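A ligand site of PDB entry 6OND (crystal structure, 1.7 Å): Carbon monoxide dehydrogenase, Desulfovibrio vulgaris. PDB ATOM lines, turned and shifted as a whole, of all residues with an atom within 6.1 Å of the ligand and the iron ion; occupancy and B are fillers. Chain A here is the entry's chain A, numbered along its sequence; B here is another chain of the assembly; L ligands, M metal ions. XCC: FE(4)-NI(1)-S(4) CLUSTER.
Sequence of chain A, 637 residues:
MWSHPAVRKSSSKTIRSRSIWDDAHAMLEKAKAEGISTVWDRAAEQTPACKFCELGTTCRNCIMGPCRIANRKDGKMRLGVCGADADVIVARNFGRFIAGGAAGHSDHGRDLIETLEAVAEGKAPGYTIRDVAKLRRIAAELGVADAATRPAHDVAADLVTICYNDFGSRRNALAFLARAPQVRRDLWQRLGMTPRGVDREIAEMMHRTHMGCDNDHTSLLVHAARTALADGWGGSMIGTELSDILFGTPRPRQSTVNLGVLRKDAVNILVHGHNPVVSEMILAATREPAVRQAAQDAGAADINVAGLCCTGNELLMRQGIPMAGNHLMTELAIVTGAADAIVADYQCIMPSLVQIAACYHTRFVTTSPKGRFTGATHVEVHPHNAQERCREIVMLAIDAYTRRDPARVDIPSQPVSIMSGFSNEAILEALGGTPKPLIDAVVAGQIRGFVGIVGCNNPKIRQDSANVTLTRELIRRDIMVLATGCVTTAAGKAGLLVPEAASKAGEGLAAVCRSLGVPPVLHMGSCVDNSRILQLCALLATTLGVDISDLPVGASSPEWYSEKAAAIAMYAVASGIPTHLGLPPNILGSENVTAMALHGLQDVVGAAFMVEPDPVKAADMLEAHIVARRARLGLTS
The side-chain sulfur of Cys 456 is bound to an iron atom (FE3) of the ligand, 2.5 Å away.
An iron atom (FE4) of the ligand is bound by the side-chain sulfur of Cys 486.
The side-chain sulfur of Cys 348 is bound to an iron atom (FE1) of the ligand.
A sulfur (S1) of the ligand lies close to the backbone NH of Cys 456 (3.8 Å).
An iron atom (FE2) of the ligand is bound by the side-chain sulfur of Cys 310 (2.4 Å).
S4 of the ligand lies close to OG of Ser 562 (3.2 Å).
A ring nitrogen (NE2) of His 274 binds an iron atom (FE2) of the ligand (2.2 Å).
The backbone NH of Cys 486 lies close to a sulfur (S1) of the ligand (3.4 Å).
A ring nitrogen (NE2) of His 274 lies close to the side-chain amino group (NZ) of Lys 564 (2.7 Å).
OG of Ser 562 is in hydrogen-bond range of N of Ala 565 (2.9 Å).
The side-chain amino group (NZ) of Lys 564 is in hydrogen-bond range of the side-chain amide oxygen (OE1) of Gln 347 (2.7 Å).
The backbone NH of Lys 564 sits close to the side-chain hydroxyl of Ser 562 (3.4 Å).
The backbone NH (N) of Tyr 561 lies close to the side-chain sulfur (SG) of Cys 456 (3.5 Å).
The backbone NH (N) of Cys 486 is in hydrogen-bond range of the backbone carbonyl oxygen (O) of Gly 455, at 3.2 Å.
The side-chain sulfur (SG) of Cys 456 lies close to the side-chain hydroxyl (OG) of Ser 562 (3.6 Å).
The side-chain sulfur (SG) of Cys 309 sits at hydrogen-bond distance from the backbone NH (N) of His 327 (3.6 Å).
O of Gly 455 lies close to S1 of the ligand (3.4 Å).
Cys 309 touches the ligand (CB to S3, 3.7 Å).
His 327 touches the ligand.
Tyr 561 touches the ligand (CE2 to S2, 3.5 Å).
Lys 564 touches the ligand.
Hydrophobic or aromatic side chains that line the ligand: His 274, His 327 and Tyr 561.
His 274 touches the iron ion.
Cys 310 touches the iron ion.
The iron ion is bound by a sulfur (S1) of the ligand, 2.3 Å away.
SG of Cys 527 is bound to the iron ion (2.5 Å).
S4 of the ligand is bound to the iron ion.
The iron ion is bound by a sulfur (S3) of the ligand, 2.7 Å away.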
ATOM      1  N   HIS A 105      29.541 -25.892 -24.793  1.00  0.00           N
ATOM      2  CA  HIS A 105      30.358 -25.825 -25.999  1.00  0.00           C
ATOM      3  C   HIS A 105      31.128 -27.110 -26.222  1.00  0.00           C
ATOM      4  O   HIS A 105      31.367 -27.494 -27.370  1.00  0.00           O
ATOM      5  CB  HIS A 105      31.307 -24.617 -25.942  1.00  0.00           C
ATOM      6  CG  HIS A 105      30.607 -23.301 -25.981  1.00  0.00           C
ATOM      7  ND1 HIS A 105      30.973 -22.231 -25.189  1.00  0.00           N
ATOM      8  CD2 HIS A 105      29.540 -22.885 -26.708  1.00  0.00           C
ATOM      9  CE1 HIS A 105      30.172 -21.205 -25.442  1.00  0.00           C
ATOM     10  NE2 HIS A 105      29.298 -21.574 -26.357  1.00  0.00           N
ATOM     11  N   GLY A 273      18.252 -23.790 -31.707  1.00  0.00           N
ATOM     12  CA  GLY A 273      19.267 -24.545 -30.993  1.00  0.00           C
ATOM     13  C   GLY A 273      20.665 -24.139 -31.460  1.00  0.00           C
ATOM     14  O   GLY A 273      20.888 -22.958 -31.728  1.00  0.00           O
ATOM     15  N   HIS A 274      21.589 -25.108 -31.583  1.00  0.00           N
ATOM     16  CA  HIS A 274      22.999 -24.756 -31.783  1.00  0.00           C
ATOM     17  C   HIS A 274      23.743 -25.552 -32.850  1.00  0.00           C
ATOM     18  O   HIS A 274      24.687 -25.012 -33.438  1.00  0.00           O
ATOM     19  CB  HIS A 274      23.758 -24.849 -30.454  1.00  0.00           C
ATOM     20  CG  HIS A 274      23.555 -23.646 -29.594  1.00  0.00           C
ATOM     21  ND1 HIS A 274      22.330 -23.325 -29.051  1.00  0.00           N
ATOM     22  CD2 HIS A 274      24.400 -22.653 -29.227  1.00  0.00           C
ATOM     23  CE1 HIS A 274      22.429 -22.187 -28.379  1.00  0.00           C
ATOM     24  NE2 HIS A 274      23.666 -21.748 -28.490  1.00  0.00           N
ATOM     25  N   CYS A 309      18.575 -18.070 -33.295  1.00  0.00           N
ATOM     26  CA  CYS A 309      19.686 -18.242 -32.342  1.00  0.00           C
ATOM     27  C   CYS A 309      20.918 -18.818 -33.057  1.00  0.00           C
ATOM     28  O   CYS A 309      21.175 -18.464 -34.220  1.00  0.00           O
ATOM     29  CB  CYS A 309      19.182 -18.996 -31.130  1.00  0.00           C
ATOM     30  SG  CYS A 309      18.006 -17.993 -30.176  1.00  0.00           S
ATOM     31  N   CYS A 310      21.675 -19.698 -32.424  1.00  0.00           N
ATOM     32  CA  CYS A 310      22.997 -20.017 -32.973  1.00  0.00           C
ATOM     33  C   CYS A 310      22.925 -20.924 -34.184  1.00  0.00           C
ATOM     34  O   CYS A 310      23.702 -20.758 -35.133  1.00  0.00           O
ATOM     35  CB  CYS A 310      23.901 -20.589 -31.899  1.00  0.00           C
ATOM     36  SG  CYS A 310      24.691 -19.220 -31.051  1.00  0.00           S
ATOM     37  N   ASN A 326      16.556 -13.562 -32.559  1.00  0.00           N
ATOM     38  CA  ASN A 326      17.438 -13.979 -31.496  1.00  0.00           C
ATOM     39  C   ASN A 326      16.624 -14.437 -30.281  1.00  0.00           C
ATOM     40  O   ASN A 326      15.415 -14.621 -30.353  1.00  0.00           O
ATOM     41  CB  ASN A 326      18.478 -12.887 -31.193  1.00  0.00           C
ATOM     42  CG  ASN A 326      17.861 -11.505 -31.009  1.00  0.00           C
ATOM     43  OD1 ASN A 326      16.636 -11.349 -31.041  1.00  0.00           O
ATOM     44  ND2 ASN A 326      18.703 -10.495 -30.790  1.00  0.00           N
ATOM     45  N   HIS A 327      17.312 -14.616 -29.153  1.00  0.00           N
ATOM     46  CA  HIS A 327      16.767 -15.291 -27.973  1.00  0.00           C
ATOM     47  C   HIS A 327      15.363 -14.797 -27.616  1.00  0.00           C
ATOM     48  O   HIS A 327      14.400 -15.587 -27.593  1.00  0.00           O
ATOM     49  CB  HIS A 327      17.771 -15.093 -26.839  1.00  0.00           C
ATOM     50  CG  HIS A 327      17.284 -15.525 -25.483  1.00  0.00           C
ATOM     51  ND1 HIS A 327      16.567 -16.674 -25.266  1.00  0.00           N
ATOM     52  CD2 HIS A 327      17.472 -14.969 -24.266  1.00  0.00           C
ATOM     53  CE1 HIS A 327      16.290 -16.792 -23.976  1.00  0.00           C
ATOM     54  NE2 HIS A 327      16.844 -15.774 -23.346  1.00  0.00           N
ATOM     55  N   GLN A 347      20.198 -26.440 -26.387  1.00  0.00           N
ATOM     56  CA  GLN A 347      20.756 -25.240 -25.783  1.00  0.00           C
ATOM     57  C   GLN A 347      19.939 -23.994 -26.122  1.00  0.00           C
ATOM     58  O   GLN A 347      19.713 -23.704 -27.307  1.00  0.00           O
ATOM     59  CB  GLN A 347      22.230 -25.022 -26.148  1.00  0.00           C
ATOM     60  CG  GLN A 347      23.123 -26.169 -25.739  1.00  0.00           C
ATOM     61  CD  GLN A 347      24.562 -25.967 -26.170  1.00  0.00           C
ATOM     62  OE1 GLN A 347      24.978 -24.860 -26.487  1.00  0.00           O
ATOM     63  NE2 GLN A 347      25.322 -27.058 -26.213  1.00  0.00           N
ATOM     64  N   CYS A 348      19.501 -23.280 -25.095  1.00  0.00           N
ATOM     65  CA  CYS A 348      18.822 -21.985 -25.213  1.00  0.00           C
ATOM     66  C   CYS A 348      17.423 -22.096 -25.765  1.00  0.00           C
ATOM     67  O   CYS A 348      16.833 -21.091 -26.183  1.00  0.00           O
ATOM     68  CB  CYS A 348      19.626 -20.952 -25.996  1.00  0.00           C
ATOM     69  SG  CYS A 348      21.234 -20.645 -25.229  1.00  0.00           S
ATOM     70  N   VAL A 454      29.234  -9.948 -28.224  1.00  0.00           N
ATOM     71  CA  VAL A 454      28.864 -11.351 -28.245  1.00  0.00           C
ATOM     72  C   VAL A 454      27.692 -11.544 -27.290  1.00  0.00           C
ATOM     73  O   VAL A 454      27.365 -10.666 -26.489  1.00  0.00           O
ATOM     74  CB  VAL A 454      30.072 -12.236 -27.845  1.00  0.00           C
ATOM     75  CG1 VAL A 454      31.306 -11.816 -28.641  1.00  0.00           C
ATOM     76  CG2 VAL A 454      30.388 -12.073 -26.373  1.00  0.00           C
ATOM     77  N   GLY A 455      27.034 -12.674 -27.411  1.00  0.00           N
ATOM     78  CA  GLY A 455      26.068 -13.042 -26.390  1.00  0.00           C
ATOM     79  C   GLY A 455      24.639 -12.624 -26.678  1.00  0.00           C
ATOM     80  O   GLY A 455      24.241 -12.312 -27.801  1.00  0.00           O
ATOM     81  N   CYS A 456      23.866 -12.582 -25.596  1.00  0.00           N
ATOM     82  CA  CYS A 456      22.442 -12.911 -25.573  1.00  0.00           C
ATOM     83  C   CYS A 456      21.541 -11.663 -25.527  1.00  0.00           C
ATOM     84  O   CYS A 456      21.962 -10.532 -25.796  1.00  0.00           O
ATOM     85  CB  CYS A 456      22.206 -13.790 -24.330  1.00  0.00           C
ATOM     86  SG  CYS A 456      23.551 -14.982 -23.802  1.00  0.00           S
ATOM     87  N   ASN A 457      20.266 -11.909 -25.214  1.00  0.00           N
ATOM     88  CA  ASN A 457      19.302 -10.958 -24.672  1.00  0.00           C
ATOM     89  C   ASN A 457      18.993 -11.393 -23.244  1.00  0.00           C
ATOM     90  O   ASN A 457      19.250 -12.538 -22.849  1.00  0.00           O
ATOM     91  CB  ASN A 457      17.957 -11.010 -25.430  1.00  0.00           C
ATOM     92  CG  ASN A 457      18.043 -10.546 -26.873  1.00  0.00           C
ATOM     93  OD1 ASN A 457      17.323 -11.077 -27.734  1.00  0.00           O
ATOM     94  ND2 ASN A 457      18.845  -9.527 -27.153  1.00  0.00           N
ATOM     95  N   THR A 484      28.957 -11.727 -32.926  1.00  0.00           N
ATOM     96  CA  THR A 484      28.609 -13.145 -32.915  1.00  0.00           C
ATOM     97  C   THR A 484      27.323 -13.350 -32.116  1.00  0.00           C
ATOM     98  O   THR A 484      26.894 -12.497 -31.336  1.00  0.00           O
ATOM     99  CB  THR A 484      29.704 -13.991 -32.276  1.00  0.00           C
ATOM    100  OG1 THR A 484      29.928 -13.529 -30.940  1.00  0.00           O
ATOM    101  CG2 THR A 484      31.028 -13.914 -33.075  1.00  0.00           C
ATOM    102  N   GLY A 485      26.735 -14.524 -32.297  1.00  0.00           N
ATOM    103  CA  GLY A 485      25.613 -14.925 -31.453  1.00  0.00           C
ATOM    104  C   GLY A 485      24.394 -14.044 -31.651  1.00  0.00           C
ATOM    105  O   GLY A 485      24.129 -13.530 -32.748  1.00  0.00           O
ATOM    106  N   CYS A 486      23.643 -13.831 -30.572  1.00  0.00           N
ATOM    107  CA  CYS A 486      22.377 -13.110 -30.700  1.00  0.00           C
ATOM    108  C   CYS A 486      22.565 -11.626 -30.962  1.00  0.00           C
ATOM    109  O   CYS A 486      21.623 -10.970 -31.387  1.00  0.00           O
ATOM    110  CB  CYS A 486      21.475 -13.389 -29.498  1.00  0.00           C
ATOM    111  SG  CYS A 486      20.737 -15.035 -29.606  1.00  0.00           S
ATOM    112  N   VAL A 487      23.776 -11.094 -30.734  1.00  0.00           N
ATOM    113  CA  VAL A 487      24.072  -9.728 -31.154  1.00  0.00           C
ATOM    114  C   VAL A 487      23.940  -9.580 -32.661  1.00  0.00           C
ATOM    115  O   VAL A 487      23.592  -8.498 -33.155  1.00  0.00           O
ATOM    116  CB  VAL A 487      25.463  -9.326 -30.653  1.00  0.00           C
ATOM    117  CG1 VAL A 487      25.865  -7.949 -31.221  1.00  0.00           C
ATOM    118  CG2 VAL A 487      25.492  -9.320 -29.147  1.00  0.00           C
ATOM    119  N   SER A 526      28.347 -17.879 -34.971  1.00  0.00           N
ATOM    120  CA  SER A 526      27.579 -18.286 -33.795  1.00  0.00           C
ATOM    121  C   SER A 526      28.421 -18.109 -32.548  1.00  0.00           C
ATOM    122  O   SER A 526      29.547 -17.581 -32.584  1.00  0.00           O
ATOM    123  CB  SER A 526      27.228 -19.763 -33.951  1.00  0.00           C
ATOM    124  OG  SER A 526      28.444 -20.508 -33.995  1.00  0.00           O
ATOM    125  N   CYS A 527      27.922 -18.609 -31.412  1.00  0.00           N
ATOM    126  CA  CYS A 527      28.640 -18.462 -30.144  1.00  0.00           C
ATOM    127  C   CYS A 527      29.905 -19.301 -30.097  1.00  0.00           C
ATOM    128  O   CYS A 527      30.903 -18.871 -29.490  1.00  0.00           O
ATOM    129  CB  CYS A 527      27.741 -18.821 -28.972  1.00  0.00           C
ATOM    130  SG  CYS A 527      26.602 -17.513 -28.643  1.00  0.00           S
ATOM    131  N   TYR A 561      22.839 -13.679 -20.653  1.00  0.00           N
ATOM    132  CA  TYR A 561      22.069 -14.435 -19.656  1.00  0.00           C
ATOM    133  C   TYR A 561      22.645 -15.801 -19.326  1.00  0.00           C
ATOM    134  O   TYR A 561      22.474 -16.272 -18.192  1.00  0.00           O
ATOM    135  CB  TYR A 561      20.588 -14.605 -20.123  1.00  0.00           C
ATOM    136  CG  TYR A 561      20.358 -15.967 -20.762  1.00  0.00           C
ATOM    137  CD1 TYR A 561      20.018 -17.076 -19.992  1.00  0.00           C
ATOM    138  CD2 TYR A 561      20.522 -16.146 -22.130  1.00  0.00           C
ATOM    139  CE1 TYR A 561      19.876 -18.325 -20.562  1.00  0.00           C
ATOM    140  CE2 TYR A 561      20.354 -17.401 -22.713  1.00  0.00           C
ATOM    141  CZ  TYR A 561      20.035 -18.487 -21.914  1.00  0.00           C
ATOM    142  OH  TYR A 561      19.897 -19.736 -22.452  1.00  0.00           O
ATOM    143  N   SER A 562      23.318 -16.473 -20.272  1.00  0.00           N
ATOM    144  CA  SER A 562      23.580 -17.906 -20.175  1.00  0.00           C
ATOM    145  C   SER A 562      24.916 -18.191 -19.502  1.00  0.00           C
ATOM    146  O   SER A 562      25.815 -17.349 -19.465  1.00  0.00           O
ATOM    147  CB  SER A 562      23.608 -18.537 -21.571  1.00  0.00           C
ATOM    148  OG  SER A 562      24.712 -18.040 -22.309  1.00  0.00           O
ATOM    149  N   LYS A 564      26.874 -20.201 -20.873  1.00  0.00           N
ATOM    150  CA  LYS A 564      27.793 -20.156 -22.015  1.00  0.00           C
ATOM    151  C   LYS A 564      28.428 -18.777 -22.180  1.00  0.00           C
ATOM    152  O   LYS A 564      29.625 -18.669 -22.439  1.00  0.00           O
ATOM    153  CB  LYS A 564      27.112 -20.620 -23.292  1.00  0.00           C
ATOM    154  CG  LYS A 564      26.877 -22.125 -23.302  1.00  0.00           C
ATOM    155  CD  LYS A 564      26.230 -22.552 -24.596  1.00  0.00           C
ATOM    156  CE  LYS A 564      24.800 -22.064 -24.614  1.00  0.00           C
ATOM    157  NZ  LYS A 564      24.201 -22.353 -25.917  1.00  0.00           N
ATOM    158  N   ALA A 565      27.626 -17.714 -22.073  1.00  0.00           N
ATOM    159  CA  ALA A 565      28.171 -16.366 -22.231  1.00  0.00           C
ATOM    160  C   ALA A 565      29.188 -16.057 -21.154  1.00  0.00           C
ATOM    161  O   ALA A 565      30.182 -15.370 -21.421  1.00  0.00           O
ATOM    162  CB  ALA A 565      27.037 -15.333 -22.197  1.00  0.00           C
ATOM    163  N   HIS B 210      22.107 -27.080 -18.474  1.00  0.00           N
ATOM    164  CA  HIS B 210      22.104 -25.690 -18.913  1.00  0.00           C
ATOM    165  C   HIS B 210      20.687 -25.301 -19.333  1.00  0.00           C
ATOM    166  O   HIS B 210      19.893 -26.148 -19.742  1.00  0.00           O
ATOM    167  CB  HIS B 210      23.086 -25.557 -20.092  1.00  0.00           C
ATOM    168  CG  HIS B 210      23.329 -24.154 -20.559  1.00  0.00           C
ATOM    169  ND1 HIS B 210      22.413 -23.424 -21.285  1.00  0.00           N
ATOM    170  CD2 HIS B 210      24.437 -23.364 -20.452  1.00  0.00           C
ATOM    171  CE1 HIS B 210      22.927 -22.238 -21.567  1.00  0.00           C
ATOM    172  NE2 HIS B 210      24.152 -22.176 -21.079  1.00  0.00           N
HETATM  173 FE1  XCC L   1      22.004 -18.632 -26.378  1.00  0.00          FE
HETATM  174 FE2  XCC L   1      23.919 -19.539 -28.810  1.00  0.00          FE
HETATM  175 FE3  XCC L   1      23.280 -16.465 -25.736  1.00  0.00          FE
HETATM  176 FE4  XCC L   1      21.911 -16.504 -28.041  1.00  0.00          FE
HETATM  177  S1  XCC L   1      24.043 -15.709 -27.742  1.00  0.00           S
HETATM  178  S2  XCC L   1      20.972 -16.651 -26.036  1.00  0.00           S
HETATM  179  S4  XCC L   1      24.109 -18.570 -25.357  1.00  0.00           S
HETATM  180  S3  XCC L   1      21.937 -18.685 -28.638  1.00  0.00           S
HETATM  181 FE    FE M   1      24.364 -17.958 -27.734  1.00  0.00          FE
